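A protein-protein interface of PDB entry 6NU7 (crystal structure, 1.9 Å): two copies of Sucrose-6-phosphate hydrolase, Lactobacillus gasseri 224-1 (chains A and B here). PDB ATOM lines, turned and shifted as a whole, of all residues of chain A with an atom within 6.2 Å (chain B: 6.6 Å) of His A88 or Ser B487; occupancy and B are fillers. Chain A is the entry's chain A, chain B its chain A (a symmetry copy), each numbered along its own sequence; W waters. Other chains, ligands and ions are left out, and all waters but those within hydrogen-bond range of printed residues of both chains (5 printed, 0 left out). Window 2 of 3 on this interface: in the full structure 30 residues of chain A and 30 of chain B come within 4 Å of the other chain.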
ATOM      1  N   GLU A  57       5.659  21.778  -9.264  1.00  0.00           N
ATOM      2  CA  GLU A  57       4.397  22.400  -8.880  1.00  0.00           C
ATOM      3  C   GLU A  57       4.586  23.905  -8.750  1.00  0.00           C
ATOM      4  O   GLU A  57       5.712  24.425  -8.705  1.00  0.00           O
ATOM      5  CB  GLU A  57       3.831  21.793  -7.586  1.00  0.00           C
ATOM      6  CG  GLU A  57       4.713  21.978  -6.380  1.00  0.00           C
ATOM      7  CD  GLU A  57       4.377  21.011  -5.227  1.00  0.00           C
ATOM      8  OE1 GLU A  57       3.222  20.550  -5.120  1.00  0.00           O
ATOM      9  OE2 GLU A  57       5.293  20.724  -4.422  1.00  0.00           O
ATOM     10  N   HIS A  78       3.989  29.239   3.424  1.00  0.00           N
ATOM     11  CA  HIS A  78       4.200  28.560   2.141  1.00  0.00           C
ATOM     12  C   HIS A  78       2.975  27.756   1.709  1.00  0.00           C
ATOM     13  O   HIS A  78       2.463  26.944   2.488  1.00  0.00           O
ATOM     14  CB  HIS A  78       5.437  27.658   2.273  1.00  0.00           C
ATOM     15  CG  HIS A  78       5.903  27.002   1.000  1.00  0.00           C
ATOM     16  ND1 HIS A  78       6.960  26.110   0.984  1.00  0.00           N
ATOM     17  CD2 HIS A  78       5.460  27.083  -0.278  1.00  0.00           C
ATOM     18  CE1 HIS A  78       7.173  25.695  -0.254  1.00  0.00           C
ATOM     19  NE2 HIS A  78       6.271  26.264  -1.037  1.00  0.00           N
ATOM     20  N   PHE A  79       2.544  27.945   0.443  1.00  0.00           N
ATOM     21  CA  PHE A  79       1.526  27.119  -0.193  1.00  0.00           C
ATOM     22  C   PHE A  79       2.067  26.586  -1.520  1.00  0.00           C
ATOM     23  O   PHE A  79       2.926  27.199  -2.148  1.00  0.00           O
ATOM     24  CB  PHE A  79       0.221  27.898  -0.516  1.00  0.00           C
ATOM     25  CG  PHE A  79      -0.544  28.383   0.695  1.00  0.00           C
ATOM     26  CD1 PHE A  79      -0.261  29.623   1.266  1.00  0.00           C
ATOM     27  CD2 PHE A  79      -1.578  27.615   1.228  1.00  0.00           C
ATOM     28  CE1 PHE A  79      -0.979  30.081   2.374  1.00  0.00           C
ATOM     29  CE2 PHE A  79      -2.293  28.064   2.335  1.00  0.00           C
ATOM     30  CZ  PHE A  79      -1.993  29.300   2.893  1.00  0.00           C
ATOM     31  N   ALA A  80       1.514  25.471  -1.975  1.00  0.00           N
ATOM     32  CA  ALA A  80       1.834  24.946  -3.299  1.00  0.00           C
ATOM     33  C   ALA A  80       0.556  24.440  -3.967  1.00  0.00           C
ATOM     34  O   ALA A  80      -0.446  24.189  -3.290  1.00  0.00           O
ATOM     35  CB  ALA A  80       2.881  23.839  -3.210  1.00  0.00           C
ATOM     36  N   SER A  81       0.619  24.236  -5.290  1.00  0.00           N
ATOM     37  CA  SER A  81      -0.568  23.862  -6.050  1.00  0.00           C
ATOM     38  C   SER A  81      -0.146  23.198  -7.348  1.00  0.00           C
ATOM     39  O   SER A  81       0.923  23.522  -7.881  1.00  0.00           O
ATOM     40  CB  SER A  81      -1.429  25.092  -6.356  1.00  0.00           C
ATOM     41  OG  SER A  81      -2.306  24.837  -7.420  1.00  0.00           O
ATOM     42  N   PRO A  82      -0.956  22.279  -7.889  1.00  0.00           N
ATOM     43  CA  PRO A  82      -0.666  21.772  -9.237  1.00  0.00           C
ATOM     44  C   PRO A  82      -1.144  22.693 -10.336  1.00  0.00           C
ATOM     45  O   PRO A  82      -0.649  22.577 -11.462  1.00  0.00           O
ATOM     46  CB  PRO A  82      -1.444  20.452  -9.294  1.00  0.00           C
ATOM     47  CG  PRO A  82      -2.690  20.737  -8.463  1.00  0.00           C
ATOM     48  CD  PRO A  82      -2.137  21.614  -7.292  1.00  0.00           C
ATOM     49  N   HIS A  86      -5.990  24.873  -6.612  1.00  0.00           N
ATOM     50  CA  HIS A  86      -6.104  23.998  -5.442  1.00  0.00           C
ATOM     51  C   HIS A  86      -4.825  24.101  -4.624  1.00  0.00           C
ATOM     52  O   HIS A  86      -3.841  23.419  -4.873  1.00  0.00           O
ATOM     53  CB  HIS A  86      -6.380  22.566  -5.876  1.00  0.00           C
ATOM     54  CG  HIS A  86      -7.691  22.407  -6.595  1.00  0.00           C
ATOM     55  ND1 HIS A  86      -7.796  22.420  -7.972  1.00  0.00           N
ATOM     56  CD2 HIS A  86      -8.949  22.215  -6.118  1.00  0.00           C
ATOM     57  CE1 HIS A  86      -9.065  22.250  -8.312  1.00  0.00           C
ATOM     58  NE2 HIS A  86      -9.787  22.133  -7.205  1.00  0.00           N
ATOM     59  N   TRP A  87      -4.831  24.965  -3.629  1.00  0.00           N
ATOM     60  CA  TRP A  87      -3.615  25.192  -2.860  1.00  0.00           C
ATOM     61  C   TRP A  87      -3.638  24.332  -1.613  1.00  0.00           C
ATOM     62  O   TRP A  87      -4.703  24.017  -1.080  1.00  0.00           O
ATOM     63  CB  TRP A  87      -3.486  26.659  -2.476  1.00  0.00           C
ATOM     64  CG  TRP A  87      -3.380  27.567  -3.647  1.00  0.00           C
ATOM     65  CD1 TRP A  87      -4.402  28.231  -4.275  1.00  0.00           C
ATOM     66  CD2 TRP A  87      -2.181  27.907  -4.354  1.00  0.00           C
ATOM     67  NE1 TRP A  87      -3.905  28.993  -5.309  1.00  0.00           N
ATOM     68  CE2 TRP A  87      -2.547  28.805  -5.389  1.00  0.00           C
ATOM     69  CE3 TRP A  87      -0.833  27.559  -4.196  1.00  0.00           C
ATOM     70  CZ2 TRP A  87      -1.613  29.370  -6.261  1.00  0.00           C
ATOM     71  CZ3 TRP A  87       0.092  28.101  -5.064  1.00  0.00           C
ATOM     72  CH2 TRP A  87      -0.298  29.013  -6.080  1.00  0.00           C
ATOM     73  N   HIS A  88      -2.453  23.930  -1.160  1.00  0.00           N
ATOM     74  CA  HIS A  88      -2.338  23.232   0.102  1.00  0.00           C
ATOM     75  C   HIS A  88      -1.231  23.894   0.914  1.00  0.00           C
ATOM     76  O   HIS A  88      -0.230  24.364   0.364  1.00  0.00           O
ATOM     77  CB  HIS A  88      -2.087  21.689  -0.097  1.00  0.00           C
ATOM     78  CG  HIS A  88      -0.831  21.342  -0.853  1.00  0.00           C
ATOM     79  ND1 HIS A  88      -0.778  21.270  -2.229  1.00  0.00           N
ATOM     80  CD2 HIS A  88       0.413  21.020  -0.420  1.00  0.00           C
ATOM     81  CE1 HIS A  88       0.442  20.928  -2.612  1.00  0.00           C
ATOM     82  NE2 HIS A  88       1.185  20.771  -1.531  1.00  0.00           N
ATOM     83  N   TYR A  89      -1.437  23.929   2.224  1.00  0.00           N
ATOM     84  CA  TYR A  89      -0.575  24.641   3.168  1.00  0.00           C
ATOM     85  C   TYR A  89       0.674  23.832   3.492  1.00  0.00           C
ATOM     86  O   TYR A  89       0.575  22.658   3.866  1.00  0.00           O
ATOM     87  CB  TYR A  89      -1.359  24.898   4.451  1.00  0.00           C
ATOM     88  CG  TYR A  89      -0.675  25.685   5.559  1.00  0.00           C
ATOM     89  CD1 TYR A  89      -0.191  26.968   5.339  1.00  0.00           C
ATOM     90  CD2 TYR A  89      -0.596  25.160   6.844  1.00  0.00           C
ATOM     91  CE1 TYR A  89       0.377  27.694   6.381  1.00  0.00           C
ATOM     92  CE2 TYR A  89      -0.045  25.872   7.888  1.00  0.00           C
ATOM     93  CZ  TYR A  89       0.437  27.122   7.655  1.00  0.00           C
ATOM     94  OH  TYR A  89       0.998  27.801   8.708  1.00  0.00           O
ATOM     95  N   LEU A  90       1.849  24.464   3.365  1.00  0.00           N
ATOM     96  CA  LEU A  90       3.107  23.833   3.738  1.00  0.00           C
ATOM     97  C   LEU A  90       3.733  24.450   4.981  1.00  0.00           C
ATOM     98  O   LEU A  90       4.859  24.086   5.324  1.00  0.00           O
ATOM     99  CB  LEU A  90       4.107  23.888   2.573  1.00  0.00           C
ATOM    100  CG  LEU A  90       3.640  23.069   1.368  1.00  0.00           C
ATOM    101  CD1 LEU A  90       4.568  23.280   0.186  1.00  0.00           C
ATOM    102  CD2 LEU A  90       3.572  21.560   1.703  1.00  0.00           C
ATOM    103  N   LEU A 489     -10.797  25.583   0.185  1.00  0.00           N
ATOM    104  CA  LEU A 489      -9.878  26.207   1.140  1.00  0.00           C
ATOM    105  C   LEU A 489     -10.591  26.682   2.400  1.00  0.00           C
ATOM    106  O   LEU A 489      -9.910  26.966   3.391  1.00  0.00           O
ATOM    107  CB  LEU A 489      -9.164  27.426   0.488  1.00  0.00           C
ATOM    108  CG  LEU A 489      -8.115  27.035  -0.561  1.00  0.00           C
ATOM    109  CD1 LEU A 489      -7.620  28.270  -1.335  1.00  0.00           C
ATOM    110  CD2 LEU A 489      -6.965  26.340   0.121  1.00  0.00           C
ATOM    111  OXT LEU A 489     -11.820  26.874   2.439  1.00  0.00           O
ATOM    112  N   ALA B  28       3.920  19.366   7.498  1.00  0.00           N
ATOM    113  CA  ALA B  28       3.452  19.587   6.125  1.00  0.00           C
ATOM    114  C   ALA B  28       4.533  19.286   5.085  1.00  0.00           C
ATOM    115  O   ALA B  28       4.213  18.799   3.991  1.00  0.00           O
ATOM    116  CB  ALA B  28       2.951  21.024   5.966  1.00  0.00           C
ATOM    117  N   HIS B  35      -0.896  14.014   0.463  1.00  0.00           N
ATOM    118  CA  HIS B  35      -1.412  15.256  -0.097  1.00  0.00           C
ATOM    119  C   HIS B  35      -2.727  15.120  -0.875  1.00  0.00           C
ATOM    120  O   HIS B  35      -3.187  16.112  -1.475  1.00  0.00           O
ATOM    121  CB  HIS B  35      -0.346  15.910  -0.972  1.00  0.00           C
ATOM    122  CG  HIS B  35       0.804  16.430  -0.178  1.00  0.00           C
ATOM    123  ND1 HIS B  35       0.670  17.476   0.710  1.00  0.00           N
ATOM    124  CD2 HIS B  35       2.087  16.012  -0.081  1.00  0.00           C
ATOM    125  CE1 HIS B  35       1.831  17.703   1.298  1.00  0.00           C
ATOM    126  NE2 HIS B  35       2.711  16.831   0.835  1.00  0.00           N
ATOM    127  N   TYR B  36      -3.383  13.958  -0.844  1.00  0.00           N
ATOM    128  CA  TYR B  36      -4.810  13.952  -1.168  1.00  0.00           C
ATOM    129  C   TYR B  36      -5.609  13.133  -0.163  1.00  0.00           C
ATOM    130  O   TYR B  36      -6.729  12.715  -0.459  1.00  0.00           O
ATOM    131  CB  TYR B  36      -5.079  13.503  -2.625  1.00  0.00           C
ATOM    132  CG  TYR B  36      -4.709  12.086  -3.078  1.00  0.00           C
ATOM    133  CD1 TYR B  36      -3.449  11.798  -3.580  1.00  0.00           C
ATOM    134  CD2 TYR B  36      -5.663  11.061  -3.087  1.00  0.00           C
ATOM    135  CE1 TYR B  36      -3.122  10.509  -4.043  1.00  0.00           C
ATOM    136  CE2 TYR B  36      -5.353   9.767  -3.547  1.00  0.00           C
ATOM    137  CZ  TYR B  36      -4.091   9.501  -4.026  1.00  0.00           C
ATOM    138  OH  TYR B  36      -3.809   8.220  -4.456  1.00  0.00           O
ATOM    139  N   HIS B  39      -4.597  14.637   6.761  1.00  0.00           N
ATOM    140  CA  HIS B  39      -3.417  14.414   7.578  1.00  0.00           C
ATOM    141  C   HIS B  39      -3.384  15.505   8.632  1.00  0.00           C
ATOM    142  O   HIS B  39      -4.057  16.531   8.478  1.00  0.00           O
ATOM    143  CB  HIS B  39      -2.141  14.451   6.730  1.00  0.00           C
ATOM    144  CG  HIS B  39      -1.908  15.769   6.055  1.00  0.00           C
ATOM    145  ND1 HIS B  39      -1.312  16.840   6.699  1.00  0.00           N
ATOM    146  CD2 HIS B  39      -2.202  16.194   4.804  1.00  0.00           C
ATOM    147  CE1 HIS B  39      -1.247  17.864   5.863  1.00  0.00           C
ATOM    148  NE2 HIS B  39      -1.766  17.493   4.704  1.00  0.00           N
ATOM    149  N   LEU B 347      -9.404  13.952  -9.038  1.00  0.00           N
ATOM    150  CA  LEU B 347      -7.971  14.128  -8.821  1.00  0.00           C
ATOM    151  C   LEU B 347      -7.134  13.600  -9.985  1.00  0.00           C
ATOM    152  O   LEU B 347      -5.956  13.967 -10.109  1.00  0.00           O
ATOM    153  CB  LEU B 347      -7.559  13.424  -7.511  1.00  0.00           C
ATOM    154  CG  LEU B 347      -8.316  13.891  -6.261  1.00  0.00           C
ATOM    155  CD1 LEU B 347      -7.732  13.283  -4.973  1.00  0.00           C
ATOM    156  CD2 LEU B 347      -8.334  15.404  -6.164  1.00  0.00           C
ATOM    157  N   HIS B 349      -5.225  12.708 -13.400  1.00  0.00           N
ATOM    158  CA  HIS B 349      -4.712  13.347 -14.607  1.00  0.00           C
ATOM    159  C   HIS B 349      -3.616  12.457 -15.203  1.00  0.00           C
ATOM    160  O   HIS B 349      -3.211  11.451 -14.615  1.00  0.00           O
ATOM    161  CB  HIS B 349      -4.194  14.764 -14.306  1.00  0.00           C
ATOM    162  CG  HIS B 349      -3.139  14.808 -13.243  1.00  0.00           C
ATOM    163  ND1 HIS B 349      -1.830  15.165 -13.509  1.00  0.00           N
ATOM    164  CD2 HIS B 349      -3.193  14.524 -11.917  1.00  0.00           C
ATOM    165  CE1 HIS B 349      -1.126  15.105 -12.390  1.00  0.00           C
ATOM    166  NE2 HIS B 349      -1.929  14.721 -11.409  1.00  0.00           N
ATOM    167  N   GLN B 367       2.033  10.151  -6.001  1.00  0.00           N
ATOM    168  CA  GLN B 367       0.579  10.209  -5.855  1.00  0.00           C
ATOM    169  C   GLN B 367      -0.047   9.672  -7.143  1.00  0.00           C
ATOM    170  O   GLN B 367       0.048  10.324  -8.192  1.00  0.00           O
ATOM    171  CB  GLN B 367       0.120  11.635  -5.577  1.00  0.00           C
ATOM    172  CG  GLN B 367       0.558  12.074  -4.179  1.00  0.00           C
ATOM    173  CD  GLN B 367       0.625  13.557  -3.999  1.00  0.00           C
ATOM    174  OE1 GLN B 367       1.364  14.050  -3.138  1.00  0.00           O
ATOM    175  NE2 GLN B 367      -0.179  14.293  -4.778  1.00  0.00           N
ATOM    176  N   ASP B 442      -0.330   7.430  -2.017  1.00  0.00           N
ATOM    177  CA  ASP B 442      -0.268   8.846  -1.641  1.00  0.00           C
ATOM    178  C   ASP B 442       0.801   8.951  -0.559  1.00  0.00           C
ATOM    179  O   ASP B 442       0.540   8.591   0.592  1.00  0.00           O
ATOM    180  CB  ASP B 442      -1.633   9.342  -1.149  1.00  0.00           C
ATOM    181  CG  ASP B 442      -1.644  10.837  -0.780  1.00  0.00           C
ATOM    182  OD1 ASP B 442      -0.666  11.576  -1.068  1.00  0.00           O
ATOM    183  OD2 ASP B 442      -2.663  11.262  -0.179  1.00  0.00           O
ATOM    184  N   MET B 485      -2.419  11.607  -9.423  1.00  0.00           N
ATOM    185  CA  MET B 485      -3.453  12.198  -8.584  1.00  0.00           C
ATOM    186  C   MET B 485      -2.948  13.527  -8.035  1.00  0.00           C
ATOM    187  O   MET B 485      -1.883  13.573  -7.404  1.00  0.00           O
ATOM    188  CB  MET B 485      -3.843  11.267  -7.438  1.00  0.00           C
ATOM    189  CG  MET B 485      -4.395   9.895  -7.904  1.00  0.00           C
ATOM    190  SD  MET B 485      -5.991   9.996  -8.743  1.00  0.00           S
ATOM    191  CE  MET B 485      -7.080   9.620  -7.376  1.00  0.00           C
ATOM    192  N   ASN B 486      -3.717  14.593  -8.261  1.00  0.00           N
ATOM    193  CA  ASN B 486      -3.281  15.939  -7.889  1.00  0.00           C
ATOM    194  C   ASN B 486      -3.291  16.124  -6.380  1.00  0.00           C
ATOM    195  O   ASN B 486      -4.171  15.615  -5.683  1.00  0.00           O
ATOM    196  CB  ASN B 486      -4.180  16.990  -8.549  1.00  0.00           C
ATOM    197  CG  ASN B 486      -3.784  17.255  -9.992  1.00  0.00           C
ATOM    198  OD1 ASN B 486      -2.585  17.278 -10.327  1.00  0.00           O
ATOM    199  ND2 ASN B 486      -4.767  17.442 -10.850  1.00  0.00           N
ATOM    200  N   SER B 487      -2.307  16.884  -5.880  1.00  0.00           N
ATOM    201  CA  SER B 487      -2.305  17.303  -4.484  1.00  0.00           C
ATOM    202  C   SER B 487      -3.386  18.355  -4.226  1.00  0.00           C
ATOM    203  O   SER B 487      -3.548  19.311  -5.001  1.00  0.00           O
ATOM    204  CB  SER B 487      -0.935  17.847  -4.092  1.00  0.00           C
ATOM    205  OG  SER B 487       0.026  16.832  -4.283  1.00  0.00           O
ATOM    206  N   ILE B 488      -4.136  18.154  -3.145  1.00  0.00           N
ATOM    207  CA  ILE B 488      -5.233  19.031  -2.734  1.00  0.00           C
ATOM    208  C   ILE B 488      -5.144  19.375  -1.246  1.00  0.00           C
ATOM    209  O   ILE B 488      -5.825  20.297  -0.772  1.00  0.00           O
ATOM    210  CB  ILE B 488      -6.586  18.374  -3.047  1.00  0.00           C
ATOM    211  CG1 ILE B 488      -6.621  16.947  -2.485  1.00  0.00           C
ATOM    212  CG2 ILE B 488      -6.862  18.419  -4.529  1.00  0.00           C
ATOM    213  CD1 ILE B 488      -8.065  16.455  -2.110  1.00  0.00           C
ATOM    214  N   LEU B 489      -4.309  18.634  -0.510  1.00  0.00           N
ATOM    215  CA  LEU B 489      -4.169  18.758   0.944  1.00  0.00           C
ATOM    216  C   LEU B 489      -2.709  18.811   1.379  1.00  0.00           C
ATOM    217  O   LEU B 489      -2.450  19.192   2.525  1.00  0.00           O
ATOM    218  CB  LEU B 489      -4.854  17.559   1.659  1.00  0.00           C
ATOM    219  CG  LEU B 489      -6.387  17.609   1.610  1.00  0.00           C
ATOM    220  CD1 LEU B 489      -6.999  16.291   2.117  1.00  0.00           C
ATOM    221  CD2 LEU B 489      -6.873  18.772   2.434  1.00  0.00           C
ATOM    222  OXT LEU B 489      -1.782  18.405   0.654  1.00  0.00           O
HETATM  223  O   HOH W   1      -3.763  22.270   3.055  1.00  0.00           O
HETATM  224  O   HOH W   2      -2.737  21.530  -3.843  1.00  0.00           O
HETATM  225  O   HOH W   3       0.234  20.245   2.487  1.00  0.00           O
HETATM  226  O   HOH W   4       2.466  18.112  -3.651  1.00  0.00           O
HETATM  227  O   HOH W   5      -5.585  22.411   1.048  1.00  0.00           O
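Of the printed residues of chain B, His A88 touches His B35, Ser B487 and Leu B489. Of the printed residues of chain A, Asn B486 touches Pro A82. Of the printed residues of chain A, Ile B488 touches Trp A87 (3.9 Å). Printed residues of chain B within 4 Å of Leu A90: Ala B28. Printed residues of chain A within 4 Å of His B35: His A88 (3.7 Å). Of the printed residues of chain B, Trp A87 touches Ile B488 (3.9 Å). Leu A489 touches none of the printed residues of chain B. Glu A57 touches none of the printed residues of chain B. The nearest residue of chain A that does not touch Ser B487 is His A86 (4.1 Å). The nearest printed residue of chain B that does not touch Leu A90 is His B35 (4.3 Å).
Water W2 lies within hydrogen-bond range of O of His A86 (2.4 Å), ND1 of His A88 (2.6 Å) and O of Ser B487 (2.6 Å). Water W5 lies within hydrogen-bond range of O of Ile B488 and O of Trp A87. Water W3 lies within hydrogen-bond range of O of Tyr A89 (2.8 Å), O of Leu B489 (2.9 Å) and ND1 of His B35 (3.3 Å). Water W4 bridges OG of Ser B487 (2.8 Å) and OE1 of Glu A57 (2.9 Å). Water W1 bridges N of Tyr A89 and O of Leu B489.
Position printed for both chains: 489.
Asn B486 touches Pro A82 (OD1 to CB, 3.5 Å). Pro A82 touches Ser B487. Ile B488 touches Trp A87 (O to O, 3.9 Å). His A88 touches His B35 (CD2 to ND1, 3.7 Å). His A88 touches Ser B487 (CE1 to CB, 3.7 Å). CB of His A88 touches C of Leu B489, 3.3 Å away. O of Tyr A89 touches CB of Ala B28, 3.6 Å away. Ala B28 touches Leu A90.
N of Leu A90 is in hydrogen-bond range of O of His A78 (2.7 Å). The backbone carbonyl oxygen of Ala A80 is in hydrogen-bond range of the backbone NH of His A88, 2.9 Å away. The side-chain carboxylate (OD1) of Asp B442 sits at hydrogen-bond distance from the backbone NH (N) of His B35 (2.9 Å). O of His B35 lies within hydrogen-bond range of N of Ile B488, 2.8 Å away. The backbone carbonyl oxygen (O) of Leu B347 sits at hydrogen-bond distance from the backbone NH (N) of Asn B486 (3.0 Å). The side-chain amide nitrogen (NE2) of Gln B367 is in hydrogen-bond range of the side-chain hydroxyl (OG) of Ser B487 (2.6 Å).
Printed residues of chain A that touch a printed residue of chain B: Pro A82, Trp A87, His A88, Tyr A89 and Leu A90. Of the 13 printed residues of chain B, 6 touch a printed residue of chain A. Hydrophobic or aromatic side chains of chain B within 4 Å of the printed part of chain A: Ala B28 and His B35. Along chain B the printed residues that touch a printed residue of chain A span positions 28 to 489. Among the printed residues, no Asp or Glu carboxylate lies within 4 Å of a Lys or Arg side-chain nitrogen of the other chain.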
